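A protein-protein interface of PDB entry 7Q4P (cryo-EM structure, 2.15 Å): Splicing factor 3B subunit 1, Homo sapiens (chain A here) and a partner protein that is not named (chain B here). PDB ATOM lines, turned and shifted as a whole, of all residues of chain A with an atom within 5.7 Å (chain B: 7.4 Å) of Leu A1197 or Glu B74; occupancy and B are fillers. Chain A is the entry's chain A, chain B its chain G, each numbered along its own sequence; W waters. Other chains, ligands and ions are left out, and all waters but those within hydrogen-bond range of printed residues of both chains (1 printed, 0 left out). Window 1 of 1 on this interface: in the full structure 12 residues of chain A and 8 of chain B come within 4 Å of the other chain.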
ATOM      1  N   PHE A1155      -1.070  17.380  10.179  1.00  0.00           N
ATOM      2  CA  PHE A1155      -0.036  16.699  10.945  1.00  0.00           C
ATOM      3  C   PHE A1155       1.140  16.182  10.116  1.00  0.00           C
ATOM      4  O   PHE A1155       2.258  16.006  10.600  1.00  0.00           O
ATOM      5  CB  PHE A1155      -0.702  15.567  11.710  1.00  0.00           C
ATOM      6  CG  PHE A1155      -1.350  16.136  12.937  1.00  0.00           C
ATOM      7  CD1 PHE A1155      -0.627  16.609  14.036  1.00  0.00           C
ATOM      8  CD2 PHE A1155      -2.727  16.214  12.962  1.00  0.00           C
ATOM      9  CE1 PHE A1155      -1.289  17.110  15.158  1.00  0.00           C
ATOM     10  CE2 PHE A1155      -3.375  16.792  14.033  1.00  0.00           C
ATOM     11  CZ  PHE A1155      -2.660  17.236  15.124  1.00  0.00           C
ATOM     12  N   GLU A1156       0.881  15.975   8.830  1.00  0.00           N
ATOM     13  CA  GLU A1156       1.924  15.632   7.888  1.00  0.00           C
ATOM     14  C   GLU A1156       2.780  16.852   7.535  1.00  0.00           C
ATOM     15  O   GLU A1156       3.983  16.693   7.366  1.00  0.00           O
ATOM     16  CB  GLU A1156       1.224  15.012   6.692  1.00  0.00           C
ATOM     17  CG  GLU A1156       2.148  14.358   5.708  1.00  0.00           C
ATOM     18  CD  GLU A1156       1.450  13.814   4.472  1.00  0.00           C
ATOM     19  OE1 GLU A1156       0.281  14.200   4.214  1.00  0.00           O
ATOM     20  OE2 GLU A1156       2.071  13.000   3.762  1.00  0.00           O
ATOM     21  N   GLU A1160       6.900  18.290  13.721  1.00  0.00           N
ATOM     22  CA  GLU A1160       7.182  18.257  15.140  1.00  0.00           C
ATOM     23  C   GLU A1160       6.325  19.255  15.903  1.00  0.00           C
ATOM     24  O   GLU A1160       6.273  19.136  17.111  1.00  0.00           O
ATOM     25  CB  GLU A1160       8.641  18.618  15.404  1.00  0.00           C
ATOM     26  CG  GLU A1160       9.647  17.578  14.971  1.00  0.00           C
ATOM     27  CD  GLU A1160      10.037  17.586  13.502  1.00  0.00           C
ATOM     28  OE1 GLU A1160      10.454  18.652  13.001  1.00  0.00           O
ATOM     29  OE2 GLU A1160       9.923  16.524  12.861  1.00  0.00           O
ATOM     30  N   VAL A1192      -3.588   9.380  12.597  1.00  0.00           N
ATOM     31  CA  VAL A1192      -2.806   8.810  13.685  1.00  0.00           C
ATOM     32  C   VAL A1192      -1.457   8.472  13.096  1.00  0.00           C
ATOM     33  O   VAL A1192      -0.437   8.709  13.699  1.00  0.00           O
ATOM     34  CB  VAL A1192      -3.458   7.520  14.200  1.00  0.00           C
ATOM     35  CG1 VAL A1192      -2.593   6.804  15.217  1.00  0.00           C
ATOM     36  CG2 VAL A1192      -4.772   7.871  14.829  1.00  0.00           C
ATOM     37  N   GLN A1193      -1.451   8.053  11.844  1.00  0.00           N
ATOM     38  CA  GLN A1193      -0.184   7.716  11.248  1.00  0.00           C
ATOM     39  C   GLN A1193       0.705   8.961  11.174  1.00  0.00           C
ATOM     40  O   GLN A1193       1.887   8.880  11.476  1.00  0.00           O
ATOM     41  CB  GLN A1193      -0.408   7.222   9.831  1.00  0.00           C
ATOM     42  CG  GLN A1193       0.925   6.966   9.159  1.00  0.00           C
ATOM     43  CD  GLN A1193       0.808   6.667   7.691  1.00  0.00           C
ATOM     44  OE1 GLN A1193      -0.032   5.886   7.249  1.00  0.00           O
ATOM     45  NE2 GLN A1193       1.643   7.326   6.905  1.00  0.00           N
ATOM     46  N   HIS A1194       0.178  10.077  10.649  1.00  0.00           N
ATOM     47  CA  HIS A1194       1.026  11.244  10.458  1.00  0.00           C
ATOM     48  C   HIS A1194       1.294  11.933  11.777  1.00  0.00           C
ATOM     49  O   HIS A1194       2.218  12.695  11.842  1.00  0.00           O
ATOM     50  CB  HIS A1194       0.326  12.316   9.638  1.00  0.00           C
ATOM     51  CG  HIS A1194       0.085  11.809   8.272  1.00  0.00           C
ATOM     52  ND1 HIS A1194       1.105  11.316   7.502  1.00  0.00           N
ATOM     53  CD2 HIS A1194      -1.059  11.606   7.593  1.00  0.00           C
ATOM     54  CE1 HIS A1194       0.615  10.859   6.375  1.00  0.00           C
ATOM     55  NE2 HIS A1194      -0.716  11.023   6.404  1.00  0.00           N
ATOM     56  N   MET A1195       0.328  11.931  12.681  1.00  0.00           N
ATOM     57  CA  MET A1195       0.583  12.502  13.981  1.00  0.00           C
ATOM     58  C   MET A1195       1.739  11.761  14.616  1.00  0.00           C
ATOM     59  O   MET A1195       2.484  12.327  15.340  1.00  0.00           O
ATOM     60  CB  MET A1195      -0.563  12.142  14.905  1.00  0.00           C
ATOM     61  CG  MET A1195      -1.352  13.303  15.403  1.00  0.00           C
ATOM     62  SD  MET A1195      -2.573  12.732  16.623  1.00  0.00           S
ATOM     63  CE  MET A1195      -3.383  14.289  16.950  1.00  0.00           C
ATOM     64  N   SER A1196       1.732  10.445  14.532  1.00  0.00           N
ATOM     65  CA  SER A1196       2.605   9.568  15.278  1.00  0.00           C
ATOM     66  C   SER A1196       4.033   9.879  14.840  1.00  0.00           C
ATOM     67  O   SER A1196       4.927   9.962  15.657  1.00  0.00           O
ATOM     68  CB  SER A1196       2.228   8.160  14.876  1.00  0.00           C
ATOM     69  OG  SER A1196       2.625   7.260  15.888  1.00  0.00           O
ATOM     70  N   LEU A1197       4.261   9.845  13.532  1.00  0.00           N
ATOM     71  CA  LEU A1197       5.580  10.143  13.005  1.00  0.00           C
ATOM     72  C   LEU A1197       6.053  11.568  13.262  1.00  0.00           C
ATOM     73  O   LEU A1197       7.264  11.784  13.279  1.00  0.00           O
ATOM     74  CB  LEU A1197       5.565   9.871  11.512  1.00  0.00           C
ATOM     75  CG  LEU A1197       5.351   8.404  11.199  1.00  0.00           C
ATOM     76  CD1 LEU A1197       5.055   8.183   9.730  1.00  0.00           C
ATOM     77  CD2 LEU A1197       6.522   7.581  11.694  1.00  0.00           C
ATOM     78  N   GLY A1198       5.126  12.531  13.351  1.00  0.00           N
ATOM     79  CA  GLY A1198       5.481  13.919  13.612  1.00  0.00           C
ATOM     80  C   GLY A1198       6.014  14.134  15.028  1.00  0.00           C
ATOM     81  O   GLY A1198       7.005  14.843  15.186  1.00  0.00           O
ATOM     82  N   VAL A1199       5.415  13.454  16.029  1.00  0.00           N
ATOM     83  CA  VAL A1199       5.720  13.707  17.437  1.00  0.00           C
ATOM     84  C   VAL A1199       6.675  12.660  18.024  1.00  0.00           C
ATOM     85  O   VAL A1199       6.877  12.611  19.231  1.00  0.00           O
ATOM     86  CB  VAL A1199       4.434  13.822  18.280  1.00  0.00           C
ATOM     87  CG1 VAL A1199       3.502  14.905  17.765  1.00  0.00           C
ATOM     88  CG2 VAL A1199       3.704  12.500  18.393  1.00  0.00           C
ATOM     89  N   TYR A1200       7.228  11.790  17.184  1.00  0.00           N
ATOM     90  CA  TYR A1200       8.219  10.816  17.618  1.00  0.00           C
ATOM     91  C   TYR A1200       9.412  11.507  18.279  1.00  0.00           C
ATOM     92  O   TYR A1200      10.017  12.379  17.660  1.00  0.00           O
ATOM     93  CB  TYR A1200       8.696  10.073  16.375  1.00  0.00           C
ATOM     94  CG  TYR A1200       9.913   9.212  16.538  1.00  0.00           C
ATOM     95  CD1 TYR A1200      10.060   8.369  17.630  1.00  0.00           C
ATOM     96  CD2 TYR A1200      10.868   9.177  15.535  1.00  0.00           C
ATOM     97  CE1 TYR A1200      11.182   7.561  17.757  1.00  0.00           C
ATOM     98  CE2 TYR A1200      11.975   8.349  15.631  1.00  0.00           C
ATOM     99  CZ  TYR A1200      12.107   7.512  16.727  1.00  0.00           C
ATOM    100  OH  TYR A1200      13.215   6.724  16.856  1.00  0.00           O
ATOM    101  N   GLU A1235       2.272   1.182  11.602  1.00  0.00           N
ATOM    102  CA  GLU A1235       3.679   1.367  11.296  1.00  0.00           C
ATOM    103  C   GLU A1235       4.192   2.655  11.934  1.00  0.00           C
ATOM    104  O   GLU A1235       5.316   2.733  12.427  1.00  0.00           O
ATOM    105  CB  GLU A1235       3.863   1.483   9.790  1.00  0.00           C
ATOM    106  CG  GLU A1235       3.835   0.150   9.082  1.00  0.00           C
ATOM    107  CD  GLU A1235       4.081   0.210   7.583  1.00  0.00           C
ATOM    108  OE1 GLU A1235       3.296   0.883   6.874  1.00  0.00           O
ATOM    109  OE2 GLU A1235       5.058  -0.414   7.129  1.00  0.00           O
ATOM    110  N   GLY A1236       3.333   3.666  11.925  1.00  0.00           N
ATOM    111  CA  GLY A1236       3.633   4.944  12.508  1.00  0.00           C
ATOM    112  C   GLY A1236       3.736   4.779  14.011  1.00  0.00           C
ATOM    113  O   GLY A1236       4.549   5.438  14.616  1.00  0.00           O
ATOM    114  N   VAL A1239       7.014   3.354  15.563  1.00  0.00           N
ATOM    115  CA  VAL A1239       8.079   4.319  15.735  1.00  0.00           C
ATOM    116  C   VAL A1239       7.841   5.162  16.983  1.00  0.00           C
ATOM    117  O   VAL A1239       8.758   5.310  17.771  1.00  0.00           O
ATOM    118  CB  VAL A1239       8.168   5.175  14.470  1.00  0.00           C
ATOM    119  CG1 VAL A1239       9.201   6.269  14.651  1.00  0.00           C
ATOM    120  CG2 VAL A1239       8.497   4.255  13.311  1.00  0.00           C
ATOM    121  N   ALA A1240       6.629   5.694  17.165  1.00  0.00           N
ATOM    122  CA  ALA A1240       6.359   6.672  18.202  1.00  0.00           C
ATOM    123  C   ALA A1240       6.125   6.042  19.576  1.00  0.00           C
ATOM    124  O   ALA A1240       6.461   6.671  20.561  1.00  0.00           O
ATOM    125  CB  ALA A1240       5.159   7.469  17.796  1.00  0.00           C
ATOM    126  N   CYS B  30       7.235  11.685  -3.126  1.00  0.00           N
ATOM    127  CA  CYS B  30       7.989  10.578  -2.570  1.00  0.00           C
ATOM    128  C   CYS B  30       7.679   9.349  -3.416  1.00  0.00           C
ATOM    129  O   CYS B  30       6.577   9.161  -3.882  1.00  0.00           O
ATOM    130  CB  CYS B  30       7.588  10.348  -1.121  1.00  0.00           C
ATOM    131  SG  CYS B  30       8.478   8.996  -0.310  1.00  0.00           S
ATOM    132  N   CYS B  33       5.532   6.723  -0.880  1.00  0.00           N
ATOM    133  CA  CYS B  33       4.205   6.979  -0.340  1.00  0.00           C
ATOM    134  C   CYS B  33       3.417   8.014  -1.148  1.00  0.00           C
ATOM    135  O   CYS B  33       2.235   8.217  -0.876  1.00  0.00           O
ATOM    136  CB  CYS B  33       4.282   7.378   1.127  1.00  0.00           C
ATOM    137  SG  CYS B  33       5.077   8.982   1.378  1.00  0.00           S
ATOM    138  N   SER B  35       3.919  11.487  -1.532  1.00  0.00           N
ATOM    139  CA  SER B  35       3.673  12.667  -0.735  1.00  0.00           C
ATOM    140  C   SER B  35       4.517  13.746  -1.356  1.00  0.00           C
ATOM    141  O   SER B  35       5.660  13.478  -1.707  1.00  0.00           O
ATOM    142  CB  SER B  35       4.113  12.515   0.695  1.00  0.00           C
ATOM    143  OG  SER B  35       3.358  11.474   1.267  1.00  0.00           O
ATOM    144  N   VAL B  37       5.401  16.259   0.501  1.00  0.00           N
ATOM    145  CA  VAL B  37       5.749  16.933   1.734  1.00  0.00           C
ATOM    146  C   VAL B  37       7.140  16.482   2.175  1.00  0.00           C
ATOM    147  O   VAL B  37       7.413  15.284   2.266  1.00  0.00           O
ATOM    148  CB  VAL B  37       4.678  16.586   2.785  1.00  0.00           C
ATOM    149  CG1 VAL B  37       4.800  17.336   4.110  1.00  0.00           C
ATOM    150  CG2 VAL B  37       3.260  16.681   2.242  1.00  0.00           C
ATOM    151  N   ARG B  38       8.016  17.458   2.469  1.00  0.00           N
ATOM    152  CA  ARG B  38       9.274  17.314   3.194  1.00  0.00           C
ATOM    153  C   ARG B  38      10.171  16.279   2.526  1.00  0.00           C
ATOM    154  O   ARG B  38      10.279  15.185   3.030  1.00  0.00           O
ATOM    155  CB  ARG B  38       9.057  16.912   4.668  1.00  0.00           C
ATOM    156  CG  ARG B  38       8.354  17.960   5.517  1.00  0.00           C
ATOM    157  CD  ARG B  38       8.660  18.068   7.010  1.00  0.00           C
ATOM    158  NE  ARG B  38       8.382  16.852   7.767  1.00  0.00           N
ATOM    159  CZ  ARG B  38       7.193  16.461   8.210  1.00  0.00           C
ATOM    160  NH1 ARG B  38       6.125  17.205   8.000  1.00  0.00           N
ATOM    161  NH2 ARG B  38       7.073  15.332   8.889  1.00  0.00           N
ATOM    162  N   CYS B  40      13.600  14.325   1.983  1.00  0.00           N
ATOM    163  CA  CYS B  40      14.642  14.122   2.964  1.00  0.00           C
ATOM    164  C   CYS B  40      15.829  13.436   2.303  1.00  0.00           C
ATOM    165  O   CYS B  40      16.826  14.071   2.008  1.00  0.00           O
ATOM    166  CB  CYS B  40      14.073  13.309   4.115  1.00  0.00           C
ATOM    167  SG  CYS B  40      15.192  13.118   5.520  1.00  0.00           S
ATOM    168  N   TYR B  71      13.088  10.370  -0.937  1.00  0.00           N
ATOM    169  CA  TYR B  71      12.146   9.771  -0.016  1.00  0.00           C
ATOM    170  C   TYR B  71      11.733  10.891   0.915  1.00  0.00           C
ATOM    171  O   TYR B  71      12.575  11.718   1.210  1.00  0.00           O
ATOM    172  CB  TYR B  71      12.906   8.756   0.827  1.00  0.00           C
ATOM    173  CG  TYR B  71      13.386   7.556   0.048  1.00  0.00           C
ATOM    174  CD1 TYR B  71      12.502   6.569  -0.377  1.00  0.00           C
ATOM    175  CD2 TYR B  71      14.737   7.382  -0.240  1.00  0.00           C
ATOM    176  CE1 TYR B  71      12.960   5.431  -1.037  1.00  0.00           C
ATOM    177  CE2 TYR B  71      15.207   6.249  -0.892  1.00  0.00           C
ATOM    178  CZ  TYR B  71      14.315   5.269  -1.298  1.00  0.00           C
ATOM    179  OH  TYR B  71      14.787   4.173  -1.975  1.00  0.00           O
ATOM    180  N   CYS B  72      10.479  10.925   1.360  1.00  0.00           N
ATOM    181  CA  CYS B  72      10.052  11.931   2.330  1.00  0.00           C
ATOM    182  C   CYS B  72      10.619  11.639   3.724  1.00  0.00           C
ATOM    183  O   CYS B  72      11.064  10.523   3.963  1.00  0.00           O
ATOM    184  CB  CYS B  72       8.530  12.019   2.359  1.00  0.00           C
ATOM    185  SG  CYS B  72       7.684  10.582   3.086  1.00  0.00           S
ATOM    186  N   LYS B  73      10.463  12.587   4.665  1.00  0.00           N
ATOM    187  CA  LYS B  73      10.889  12.438   6.043  1.00  0.00           C
ATOM    188  C   LYS B  73      10.160  11.278   6.702  1.00  0.00           C
ATOM    189  O   LYS B  73      10.743  10.571   7.489  1.00  0.00           O
ATOM    190  CB  LYS B  73      10.637  13.698   6.866  1.00  0.00           C
ATOM    191  CG  LYS B  73      11.711  14.750   6.682  1.00  0.00           C
ATOM    192  CD  LYS B  73      11.687  15.826   7.745  1.00  0.00           C
ATOM    193  CE  LYS B  73      12.787  16.855   7.580  1.00  0.00           C
ATOM    194  NZ  LYS B  73      12.748  17.874   8.655  1.00  0.00           N
ATOM    195  N   GLU B  74       8.864  11.124   6.436  1.00  0.00           N
ATOM    196  CA  GLU B  74       8.172   9.999   7.044  1.00  0.00           C
ATOM    197  C   GLU B  74       8.719   8.656   6.576  1.00  0.00           C
ATOM    198  O   GLU B  74       8.783   7.712   7.367  1.00  0.00           O
ATOM    199  CB  GLU B  74       6.695  10.034   6.727  1.00  0.00           C
ATOM    200  CG  GLU B  74       6.010  11.043   7.601  1.00  0.00           C
ATOM    201  CD  GLU B  74       4.494  11.083   7.544  1.00  0.00           C
ATOM    202  OE1 GLU B  74       3.910  12.005   8.163  1.00  0.00           O
ATOM    203  OE2 GLU B  74       3.890  10.197   6.895  1.00  0.00           O
ATOM    204  N   CYS B  75       9.007   8.516   5.272  1.00  0.00           N
ATOM    205  CA  CYS B  75       9.585   7.264   4.787  1.00  0.00           C
ATOM    206  C   CYS B  75      10.996   7.051   5.355  1.00  0.00           C
ATOM    207  O   CYS B  75      11.460   5.934   5.501  1.00  0.00           O
ATOM    208  CB  CYS B  75       9.516   7.211   3.261  1.00  0.00           C
ATOM    209  SG  CYS B  75       7.812   6.941   2.703  1.00  0.00           S
ATOM    210  N   THR B  76      11.701   8.136   5.655  1.00  0.00           N
ATOM    211  CA  THR B  76      13.042   8.035   6.181  1.00  0.00           C
ATOM    212  C   THR B  76      12.968   7.613   7.645  1.00  0.00           C
ATOM    213  O   THR B  76      13.806   6.862   8.088  1.00  0.00           O
ATOM    214  CB  THR B  76      13.691   9.413   6.107  1.00  0.00           C
ATOM    215  OG1 THR B  76      13.800   9.693   4.714  1.00  0.00           O
ATOM    216  CG2 THR B  76      15.046   9.469   6.769  1.00  0.00           C
ATOM    217  N   ILE B  77      12.104   8.234   8.443  1.00  0.00           N
ATOM    218  CA  ILE B  77      11.975   7.786   9.822  1.00  0.00           C
ATOM    219  C   ILE B  77      11.644   6.295   9.906  1.00  0.00           C
ATOM    220  O   ILE B  77      12.161   5.598  10.773  1.00  0.00           O
ATOM    221  CB  ILE B  77      10.877   8.632  10.458  1.00  0.00           C
ATOM    222  CG1 ILE B  77      11.378  10.062  10.632  1.00  0.00           C
ATOM    223  CG2 ILE B  77      10.395   8.042  11.778  1.00  0.00           C
ATOM    224  CD1 ILE B  77      10.280  11.028  10.915  1.00  0.00           C
ATOM    225  N   GLN B  78      10.760   5.816   9.025  1.00  0.00           N
ATOM    226  CA  GLN B  78      10.333   4.422   9.006  1.00  0.00           C
ATOM    227  C   GLN B  78      11.387   3.501   8.391  1.00  0.00           C
ATOM    228  O   GLN B  78      11.211   2.282   8.408  1.00  0.00           O
ATOM    229  CB  GLN B  78       9.006   4.312   8.270  1.00  0.00           C
ATOM    230  CG  GLN B  78       7.938   5.006   9.090  1.00  0.00           C
ATOM    231  CD  GLN B  78       6.624   4.988   8.365  1.00  0.00           C
ATOM    232  OE1 GLN B  78       6.473   5.548   7.277  1.00  0.00           O
ATOM    233  NE2 GLN B  78       5.689   4.214   8.884  1.00  0.00           N
ATOM    234  N   GLU B  79      12.478   4.079   7.862  1.00  0.00           N
ATOM    235  CA  GLU B  79      13.540   3.320   7.214  1.00  0.00           C
ATOM    236  C   GLU B  79      13.018   2.650   5.946  1.00  0.00           C
ATOM    237  O   GLU B  79      13.473   1.586   5.593  1.00  0.00           O
ATOM    238  CB  GLU B  79      14.238   2.369   8.198  1.00  0.00           C
ATOM    239  CG  GLU B  79      15.135   3.095   9.224  1.00  0.00           C
ATOM    240  CD  GLU B  79      16.170   2.422  10.137  1.00  0.00           C
ATOM    241  OE1 GLU B  79      16.697   3.107  11.078  1.00  0.00           O
ATOM    242  OE2 GLU B  79      16.473   1.226   9.912  1.00  0.00           O
ATOM    243  N   LYS B  80      12.091   3.294   5.233  1.00  0.00           N
ATOM    244  CA  LYS B  80      11.546   2.730   4.005  1.00  0.00           C
ATOM    245  C   LYS B  80      12.483   3.011   2.834  1.00  0.00           C
ATOM    246  O   LYS B  80      12.321   2.480   1.750  1.00  0.00           O
ATOM    247  CB  LYS B  80      10.129   3.241   3.743  1.00  0.00           C
ATOM    248  CG  LYS B  80       9.060   2.691   4.672  1.00  0.00           C
ATOM    249  CD  LYS B  80       7.772   3.397   4.371  1.00  0.00           C
ATOM    250  CE  LYS B  80       6.533   2.921   5.094  1.00  0.00           C
ATOM    251  NZ  LYS B  80       5.387   3.786   4.728  1.00  0.00           N
HETATM  252  O   HOH W   1       3.006   4.351   8.131  1.00  0.00           O
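The side-chain carboxylate (OE2) of Glu A1156 sits at hydrogen-bond distance from the side-chain hydroxyl (OG) of Ser B35. OE1 of Glu B74 is in hydrogen-bond range of ND1 of His A1194 (3.0 Å). O of Glu A1156 lies close to NH1 of Arg B38 (2.3 Å).
O of Gly A1236 sits at hydrogen-bond distance from OG of Ser A1196, at 2.9 Å. The backbone carbonyl oxygen of Ser B35 sits at hydrogen-bond distance from the backbone NH of Cys B30 (2.8 Å). The side-chain sulfur (SG) of Cys B33 lies close to the side-chain hydroxyl (OG) of Ser B35 (3.0 Å). The backbone NH of Lys B73 lies within hydrogen-bond range of the backbone carbonyl oxygen of Arg B38, at 3.1 Å. O of Glu B74 lies close to OE1 of Gln B78 (3.2 Å). The side-chain amide oxygen (OE1) of Gln B78 sits at hydrogen-bond distance from the side-chain amino group (NZ) of Lys B80 (3.3 Å).
Of the 16 printed residues of chain A, 8 touch a printed residue of chain B. Printed residues of chain A that touch a printed residue of chain B: Glu A1156, Gln A1193, His A1194, Leu A1197, Tyr A1200, Glu A1235, Gly A1236 and Val A1239. Hydrophobic or aromatic side chains of chain A within 4 Å of the printed part of chain B: His A1194, Leu A1197, Tyr A1200 and Val A1239. Along chain A the printed residues that touch a printed residue of chain B span positions 1156 to 1239. Printed residues of chain B that touch a printed residue of chain A: Ser B35, Val B37, Arg B38, Glu B74, Ile B77 and Gln B78. Hydrophobic or aromatic side chains of chain B that line the printed part of chain A: Val B37 and Ile B77.
Printed residues of chain B within 4 Å of Glu A1156: Ser B35 (3.2 Å), Val B37 (3.4 Å), Arg B38 (2.3 Å) and Glu B74 (3.8 Å). Of the printed residues of chain B, Gly A1236 touches Gln B78 (3.9 Å). Of the printed residues of chain B, His A1194 touches Glu B74. The nearest residue of chain A that does not touch Glu B74 is Phe A1155 (5.0 Å).
Among the printed residues, pairs that only touch across the chains: Glu A1235 with Gln B78 (3.4 Å), Glu A1156 with Val B37 (3.4 Å), Val A1239 with Ile B77 (3.6 Å), Gln A1193 with Glu B74 (3.6 Å), Leu A1197 with Glu B74 (3.7 Å), Leu A1197 with Gln B78 (3.8 Å), Glu A1156 with Glu B74 (3.8 Å), Gly A1236 with Gln B78 (3.9 Å), Leu A1197 with Ile B77 (3.9 Å) and Tyr A1200 with Ile B77 (3.95 Å).
Water W1 lies within hydrogen-bond range of the side-chain amide nitrogen of Gln B78 (2.8 Å) and the side-chain amide nitrogen of Gln A1193 (3.5 Å).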
